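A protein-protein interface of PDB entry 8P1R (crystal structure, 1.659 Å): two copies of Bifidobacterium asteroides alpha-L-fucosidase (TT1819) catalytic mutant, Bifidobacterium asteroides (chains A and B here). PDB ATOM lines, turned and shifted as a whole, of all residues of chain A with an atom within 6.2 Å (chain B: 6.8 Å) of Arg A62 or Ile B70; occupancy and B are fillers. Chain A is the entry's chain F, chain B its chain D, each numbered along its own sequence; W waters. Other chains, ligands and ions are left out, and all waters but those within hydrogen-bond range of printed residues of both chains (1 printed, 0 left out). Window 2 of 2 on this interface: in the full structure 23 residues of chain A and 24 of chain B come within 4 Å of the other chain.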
ATOM      1  N   ASN A  57     -12.058  12.506  12.678  1.00  0.00           N
ATOM      2  CA  ASN A  57     -11.436  12.838  11.422  1.00  0.00           C
ATOM      3  C   ASN A  57     -12.468  12.872  10.273  1.00  0.00           C
ATOM      4  O   ASN A  57     -12.415  13.771   9.446  1.00  0.00           O
ATOM      5  CB  ASN A  57     -10.280  11.910  11.095  1.00  0.00           C
ATOM      6  CG  ASN A  57      -9.038  12.208  11.920  1.00  0.00           C
ATOM      7  OD1 ASN A  57      -8.830  13.323  12.377  1.00  0.00           O
ATOM      8  ND2 ASN A  57      -8.174  11.240  12.119  1.00  0.00           N
ATOM      9  N   LYS A  58     -13.379  11.893  10.237  1.00  0.00           N
ATOM     10  CA  LYS A  58     -14.388  11.848   9.175  1.00  0.00           C
ATOM     11  C   LYS A  58     -15.170  13.164   9.117  1.00  0.00           C
ATOM     12  O   LYS A  58     -15.445  13.687   8.026  1.00  0.00           O
ATOM     13  CB  LYS A  58     -15.323  10.643   9.352  1.00  0.00           C
ATOM     14  CG  LYS A  58     -16.318  10.401   8.212  1.00  0.00           C
ATOM     15  CD  LYS A  58     -17.243   9.211   8.438  1.00  0.00           C
ATOM     16  CE  LYS A  58     -18.434   9.177   7.489  1.00  0.00           C
ATOM     17  NZ  LYS A  58     -19.283   7.941   7.661  1.00  0.00           N
ATOM     18  N   GLU A  59     -15.519  13.725  10.298  1.00  0.00           N
ATOM     19  CA  GLU A  59     -16.262  14.965  10.340  1.00  0.00           C
ATOM     20  C   GLU A  59     -15.358  16.144  10.033  1.00  0.00           C
ATOM     21  O   GLU A  59     -15.759  17.046   9.301  1.00  0.00           O
ATOM     22  CB  GLU A  59     -16.930  15.139  11.715  1.00  0.00           C
ATOM     23  CG  GLU A  59     -18.078  14.134  11.943  1.00  0.00           C
ATOM     24  CD  GLU A  59     -19.096  14.158  10.815  1.00  0.00           C
ATOM     25  OE1 GLU A  59     -19.611  15.272  10.497  1.00  0.00           O
ATOM     26  OE2 GLU A  59     -19.293  13.088  10.154  1.00  0.00           O
ATOM     27  N   TYR A  60     -14.170  16.174  10.662  1.00  0.00           N
ATOM     28  CA  TYR A  60     -13.288  17.323  10.497  1.00  0.00           C
ATOM     29  C   TYR A  60     -12.886  17.508   9.025  1.00  0.00           C
ATOM     30  O   TYR A  60     -12.793  18.618   8.537  1.00  0.00           O
ATOM     31  CB  TYR A  60     -12.064  17.109  11.390  1.00  0.00           C
ATOM     32  CG  TYR A  60     -11.175  18.316  11.611  1.00  0.00           C
ATOM     33  CD1 TYR A  60     -11.512  19.279  12.538  1.00  0.00           C
ATOM     34  CD2 TYR A  60     -10.001  18.467  10.916  1.00  0.00           C
ATOM     35  CE1 TYR A  60     -10.692  20.350  12.814  1.00  0.00           C
ATOM     36  CE2 TYR A  60      -9.159  19.560  11.145  1.00  0.00           C
ATOM     37  CZ  TYR A  60      -9.509  20.502  12.103  1.00  0.00           C
ATOM     38  OH  TYR A  60      -8.650  21.526  12.450  1.00  0.00           O
ATOM     39  N   GLU A  61     -12.660  16.394   8.333  1.00  0.00           N
ATOM     40  CA  GLU A  61     -12.250  16.438   6.941  1.00  0.00           C
ATOM     41  C   GLU A  61     -13.284  17.137   6.051  1.00  0.00           C
ATOM     42  O   GLU A  61     -12.954  17.618   4.974  1.00  0.00           O
ATOM     43  CB  GLU A  61     -12.008  15.035   6.388  1.00  0.00           C
ATOM     44  CG  GLU A  61     -10.747  14.411   6.925  1.00  0.00           C
ATOM     45  CD  GLU A  61     -10.608  12.918   6.653  1.00  0.00           C
ATOM     46  OE1 GLU A  61     -11.363  12.419   5.725  1.00  0.00           O
ATOM     47  OE2 GLU A  61      -9.774  12.299   7.347  1.00  0.00           O
ATOM     48  N   ARG A  62     -14.550  17.171   6.444  1.00  0.00           N
ATOM     49  CA  ARG A  62     -15.566  17.861   5.668  1.00  0.00           C
ATOM     50  C   ARG A  62     -15.244  19.343   5.455  1.00  0.00           C
ATOM     51  O   ARG A  62     -15.667  19.899   4.456  1.00  0.00           O
ATOM     52  CB  ARG A  62     -16.945  17.723   6.311  1.00  0.00           C
ATOM     53  CG  ARG A  62     -17.495  16.303   6.321  1.00  0.00           C
ATOM     54  CD  ARG A  62     -18.833  16.277   7.065  1.00  0.00           C
ATOM     55  NE  ARG A  62     -19.887  16.942   6.304  1.00  0.00           N
ATOM     56  CZ  ARG A  62     -20.543  18.050   6.671  1.00  0.00           C
ATOM     57  NH1 ARG A  62     -20.225  18.696   7.773  1.00  0.00           N
ATOM     58  NH2 ARG A  62     -21.514  18.534   5.915  1.00  0.00           N
ATOM     59  N   LEU A  63     -14.440  19.928   6.328  1.00  0.00           N
ATOM     60  CA  LEU A  63     -14.027  21.318   6.230  1.00  0.00           C
ATOM     61  C   LEU A  63     -13.257  21.563   4.952  1.00  0.00           C
ATOM     62  O   LEU A  63     -13.274  22.689   4.451  1.00  0.00           O
ATOM     63  CB  LEU A  63     -13.186  21.683   7.458  1.00  0.00           C
ATOM     64  CG  LEU A  63     -13.970  21.777   8.755  1.00  0.00           C
ATOM     65  CD1 LEU A  63     -12.987  21.747   9.924  1.00  0.00           C
ATOM     66  CD2 LEU A  63     -14.760  23.056   8.752  1.00  0.00           C
ATOM     67  N   THR A  64     -12.604  20.532   4.405  1.00  0.00           N
ATOM     68  CA  THR A  64     -11.863  20.746   3.178  1.00  0.00           C
ATOM     69  C   THR A  64     -12.747  21.339   2.095  1.00  0.00           C
ATOM     70  O   THR A  64     -12.273  22.114   1.281  1.00  0.00           O
ATOM     71  CB  THR A  64     -11.207  19.454   2.658  1.00  0.00           C
ATOM     72  OG1 THR A  64     -12.180  18.454   2.377  1.00  0.00           O
ATOM     73  CG2 THR A  64     -10.147  18.923   3.600  1.00  0.00           C
ATOM     74  N   GLN A  65     -14.026  20.911   2.040  1.00  0.00           N
ATOM     75  CA  GLN A  65     -14.897  21.306   0.949  1.00  0.00           C
ATOM     76  C   GLN A  65     -15.354  22.734   1.105  1.00  0.00           C
ATOM     77  O   GLN A  65     -15.888  23.308   0.144  1.00  0.00           O
ATOM     78  CB  GLN A  65     -16.045  20.303   0.818  1.00  0.00           C
ATOM     79  CG  GLN A  65     -15.511  18.895   0.500  1.00  0.00           C
ATOM     80  CD  GLN A  65     -14.501  18.864  -0.641  1.00  0.00           C
ATOM     81  OE1 GLN A  65     -13.304  18.617  -0.430  1.00  0.00           O
ATOM     82  NE2 GLN A  65     -14.940  19.204  -1.834  1.00  0.00           N
ATOM     83  N   ALA A  66     -15.215  23.316   2.292  1.00  0.00           N
ATOM     84  CA  ALA A  66     -15.612  24.686   2.548  1.00  0.00           C
ATOM     85  C   ALA A  66     -14.435  25.663   2.453  1.00  0.00           C
ATOM     86  O   ALA A  66     -14.616  26.852   2.671  1.00  0.00           O
ATOM     87  CB  ALA A  66     -16.218  24.800   3.939  1.00  0.00           C
ATOM     88  N   ASN B  68     -20.154  27.856   0.467  1.00  0.00           N
ATOM     89  CA  ASN B  68     -20.387  26.426   0.571  1.00  0.00           C
ATOM     90  C   ASN B  68     -20.586  26.037   2.023  1.00  0.00           C
ATOM     91  O   ASN B  68     -19.728  25.421   2.641  1.00  0.00           O
ATOM     92  CB  ASN B  68     -19.281  25.608  -0.074  1.00  0.00           C
ATOM     93  CG  ASN B  68     -19.700  24.168  -0.259  1.00  0.00           C
ATOM     94  OD1 ASN B  68     -20.905  23.857  -0.274  1.00  0.00           O
ATOM     95  ND2 ASN B  68     -18.731  23.264  -0.285  1.00  0.00           N
ATOM     96  N   PRO B  69     -21.733  26.434   2.609  1.00  0.00           N
ATOM     97  CA  PRO B  69     -21.984  26.257   4.046  1.00  0.00           C
ATOM     98  C   PRO B  69     -22.329  24.831   4.442  1.00  0.00           C
ATOM     99  O   PRO B  69     -23.502  24.451   4.585  1.00  0.00           O
ATOM    100  CB  PRO B  69     -23.152  27.221   4.329  1.00  0.00           C
ATOM    101  CG  PRO B  69     -23.888  27.290   2.965  1.00  0.00           C
ATOM    102  CD  PRO B  69     -22.767  27.266   1.963  1.00  0.00           C
ATOM    103  N   ILE B  70     -21.271  24.050   4.669  1.00  0.00           N
ATOM    104  CA  ILE B  70     -21.382  22.629   4.951  1.00  0.00           C
ATOM    105  C   ILE B  70     -22.138  22.364   6.252  1.00  0.00           C
ATOM    106  O   ILE B  70     -22.478  21.207   6.471  1.00  0.00           O
ATOM    107  CB  ILE B  70     -20.009  21.955   4.973  1.00  0.00           C
ATOM    108  CG1 ILE B  70     -19.104  22.513   6.078  1.00  0.00           C
ATOM    109  CG2 ILE B  70     -19.305  22.066   3.614  1.00  0.00           C
ATOM    110  CD1 ILE B  70     -17.807  21.690   6.281  1.00  0.00           C
ATOM    111  N   TYR B  71     -22.347  23.336   7.133  1.00  0.00           N
ATOM    112  CA  TYR B  71     -23.037  23.073   8.396  1.00  0.00           C
ATOM    113  C   TYR B  71     -24.495  23.550   8.393  1.00  0.00           C
ATOM    114  O   TYR B  71     -25.190  23.374   9.397  1.00  0.00           O
ATOM    115  CB  TYR B  71     -22.256  23.694   9.583  1.00  0.00           C
ATOM    116  CG  TYR B  71     -20.925  23.018   9.776  1.00  0.00           C
ATOM    117  CD1 TYR B  71     -20.860  21.671  10.135  1.00  0.00           C
ATOM    118  CD2 TYR B  71     -19.736  23.697   9.571  1.00  0.00           C
ATOM    119  CE1 TYR B  71     -19.659  21.012  10.262  1.00  0.00           C
ATOM    120  CE2 TYR B  71     -18.515  23.048   9.750  1.00  0.00           C
ATOM    121  CZ  TYR B  71     -18.479  21.711  10.070  1.00  0.00           C
ATOM    122  OH  TYR B  71     -17.272  21.045  10.173  1.00  0.00           O
ATOM    123  N   PHE B  72     -24.981  24.116   7.288  1.00  0.00           N
ATOM    124  CA  PHE B  72     -26.373  24.510   7.206  1.00  0.00           C
ATOM    125  C   PHE B  72     -27.275  23.296   7.357  1.00  0.00           C
ATOM    126  O   PHE B  72     -27.105  22.301   6.645  1.00  0.00           O
ATOM    127  CB  PHE B  72     -26.671  25.198   5.881  1.00  0.00           C
ATOM    128  CG  PHE B  72     -28.115  25.615   5.743  1.00  0.00           C
ATOM    129  CD1 PHE B  72     -28.611  26.635   6.548  1.00  0.00           C
ATOM    130  CD2 PHE B  72     -28.975  24.919   4.923  1.00  0.00           C
ATOM    131  CE1 PHE B  72     -29.929  27.011   6.464  1.00  0.00           C
ATOM    132  CE2 PHE B  72     -30.318  25.274   4.854  1.00  0.00           C
ATOM    133  CZ  PHE B  72     -30.782  26.340   5.589  1.00  0.00           C
ATOM    134  N   ASP B  73     -28.227  23.373   8.295  1.00  0.00           N
ATOM    135  CA  ASP B  73     -29.126  22.273   8.571  1.00  0.00           C
ATOM    136  C   ASP B  73     -30.480  22.869   8.955  1.00  0.00           C
ATOM    137  O   ASP B  73     -30.689  23.289  10.091  1.00  0.00           O
ATOM    138  CB  ASP B  73     -28.566  21.371   9.679  1.00  0.00           C
ATOM    139  CG  ASP B  73     -29.441  20.149   9.961  1.00  0.00           C
ATOM    140  OD1 ASP B  73     -30.634  20.152   9.594  1.00  0.00           O
ATOM    141  OD2 ASP B  73     -28.958  19.265  10.641  1.00  0.00           O
ATOM    142  N   PHE B 117     -22.701  25.610  -3.425  1.00  0.00           N
ATOM    143  CA  PHE B 117     -23.681  24.994  -2.537  1.00  0.00           C
ATOM    144  C   PHE B 117     -24.838  24.380  -3.330  1.00  0.00           C
ATOM    145  O   PHE B 117     -25.262  23.264  -3.046  1.00  0.00           O
ATOM    146  CB  PHE B 117     -24.182  26.040  -1.525  1.00  0.00           C
ATOM    147  CG  PHE B 117     -24.920  25.445  -0.342  1.00  0.00           C
ATOM    148  CD1 PHE B 117     -24.311  24.446   0.440  1.00  0.00           C
ATOM    149  CD2 PHE B 117     -26.186  25.882  -0.002  1.00  0.00           C
ATOM    150  CE1 PHE B 117     -24.966  23.939   1.563  1.00  0.00           C
ATOM    151  CE2 PHE B 117     -26.842  25.354   1.121  1.00  0.00           C
ATOM    152  CZ  PHE B 117     -26.227  24.389   1.900  1.00  0.00           C
ATOM    153  N   ARG B 119     -27.959  24.571  -3.678  1.00  0.00           N
ATOM    154  CA  ARG B 119     -29.128  24.129  -2.924  1.00  0.00           C
ATOM    155  C   ARG B 119     -30.063  25.305  -2.705  1.00  0.00           C
ATOM    156  O   ARG B 119     -29.601  26.435  -2.546  1.00  0.00           O
ATOM    157  CB  ARG B 119     -28.695  23.497  -1.592  1.00  0.00           C
ATOM    158  CG  ARG B 119     -28.090  22.122  -1.717  1.00  0.00           C
ATOM    159  CD  ARG B 119     -27.273  21.681  -0.532  1.00  0.00           C
ATOM    160  NE  ARG B 119     -28.032  21.636   0.721  1.00  0.00           N
ATOM    161  CZ  ARG B 119     -27.529  21.315   1.898  1.00  0.00           C
ATOM    162  NH1 ARG B 119     -26.291  20.873   1.986  1.00  0.00           N
ATOM    163  NH2 ARG B 119     -28.258  21.467   3.005  1.00  0.00           N
ATOM    164  N   GLY B 330     -21.080  32.176   7.789  1.00  0.00           N
ATOM    165  CA  GLY B 330     -20.770  31.752   6.437  1.00  0.00           C
ATOM    166  C   GLY B 330     -20.806  30.253   6.235  1.00  0.00           C
ATOM    167  O   GLY B 330     -20.849  29.791   5.078  1.00  0.00           O
ATOM    168  N   LEU B 331     -20.767  29.485   7.335  1.00  0.00           N
ATOM    169  CA  LEU B 331     -20.888  28.036   7.240  1.00  0.00           C
ATOM    170  C   LEU B 331     -22.336  27.570   7.447  1.00  0.00           C
ATOM    171  O   LEU B 331     -22.568  26.360   7.452  1.00  0.00           O
ATOM    172  CB  LEU B 331     -19.990  27.390   8.285  1.00  0.00           C
ATOM    173  CG  LEU B 331     -18.489  27.502   8.005  1.00  0.00           C
ATOM    174  CD1 LEU B 331     -17.711  26.995   9.179  1.00  0.00           C
ATOM    175  CD2 LEU B 331     -18.088  26.731   6.772  1.00  0.00           C
ATOM    176  N   GLY B 332     -23.261  28.508   7.657  1.00  0.00           N
ATOM    177  CA  GLY B 332     -24.666  28.198   7.829  1.00  0.00           C
ATOM    178  C   GLY B 332     -25.074  27.897   9.272  1.00  0.00           C
ATOM    179  O   GLY B 332     -26.159  27.381   9.500  1.00  0.00           O
HETATM  180  O   HOH W   1     -17.822  18.504   9.897  1.00  0.00           O
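The backbone carbonyl oxygen (O) of Gln A65 sits at hydrogen-bond distance from the side-chain amide nitrogen (ND2) of Asn B68, 2.9 Å away.
O of Ile B70 sits at hydrogen-bond distance from NH2 of Arg A62 (2.9 Å).
The backbone NH (N) of Tyr B71 sits at hydrogen-bond distance from the backbone carbonyl oxygen (O) of Leu B331 (3.0 Å).
The backbone NH of Phe B72 sits at hydrogen-bond distance from the backbone carbonyl oxygen of Leu B331 (3.3 Å).
The side-chain hydroxyl (OG1) of Thr A64 sits at hydrogen-bond distance from the side-chain amide oxygen (OE1) of Gln A65 (3.0 Å).
Arg A62 touches Tyr B71 (NH1 to CE1, 3.4 Å).
Leu A63 touches Ile B70 (CA to CD1, 3.8 Å).
CD2 of Leu A63 touches OH of Tyr B71, 3.5 Å away.
CB of Ala A66 touches O of Asn B68, at 3.8 Å.
Ala A66 touches Leu B331 (CB to CD2, 3.9 Å).
Arg A62 touches just these residues of chain B: Ile B70 (2.9 Å) and Tyr B71 (3.4 Å).
Of the printed residues of chain A, Ile B70 touches Arg A62 (2.9 Å) and Leu A63 (3.8 Å).
Of the printed residues of chain A, Tyr B71 touches Arg A62 (3.4 Å) and Leu A63 (3.5 Å).
Of the printed residues of chain B, Leu A63 touches Ile B70 and Tyr B71.
Of the printed residues of chain A, Asn B68 touches Gln A65 and Ala A66.
Printed residues of chain B within 4 Å of Gln A65: Asn B68.
Printed residues of chain A within 4 Å of Leu B331: Ala A66 (3.9 Å).
Pro B69 touches none of the printed residues of chain A.
Gly B332 touches none of the printed residues of chain A.
The nearest residue of chain B that does not touch Arg A62 is Pro B69 (6.4 Å).
Of the 11 printed residues of chain B, 4 touch a printed residue of chain A.
Hydrophobic or aromatic side chains of chain B that line the printed part of chain A: Ile B70, Tyr B71 and Leu B331.
Of the 10 printed residues of chain A, 4 touch a printed residue of chain B.
Among the printed residues, no Asp or Glu carboxylate lies within 4 Å of a Lys or Arg side-chain nitrogen of the other chain.
No position is printed for both chains.
Of the 7 pairs that touch across the chains among the printed residues, none has its exchanged pair printed and touching as well.
Water W1 lies within hydrogen-bond range of O of Glu A59, OH of Tyr B71 and NH1 of Arg A62.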
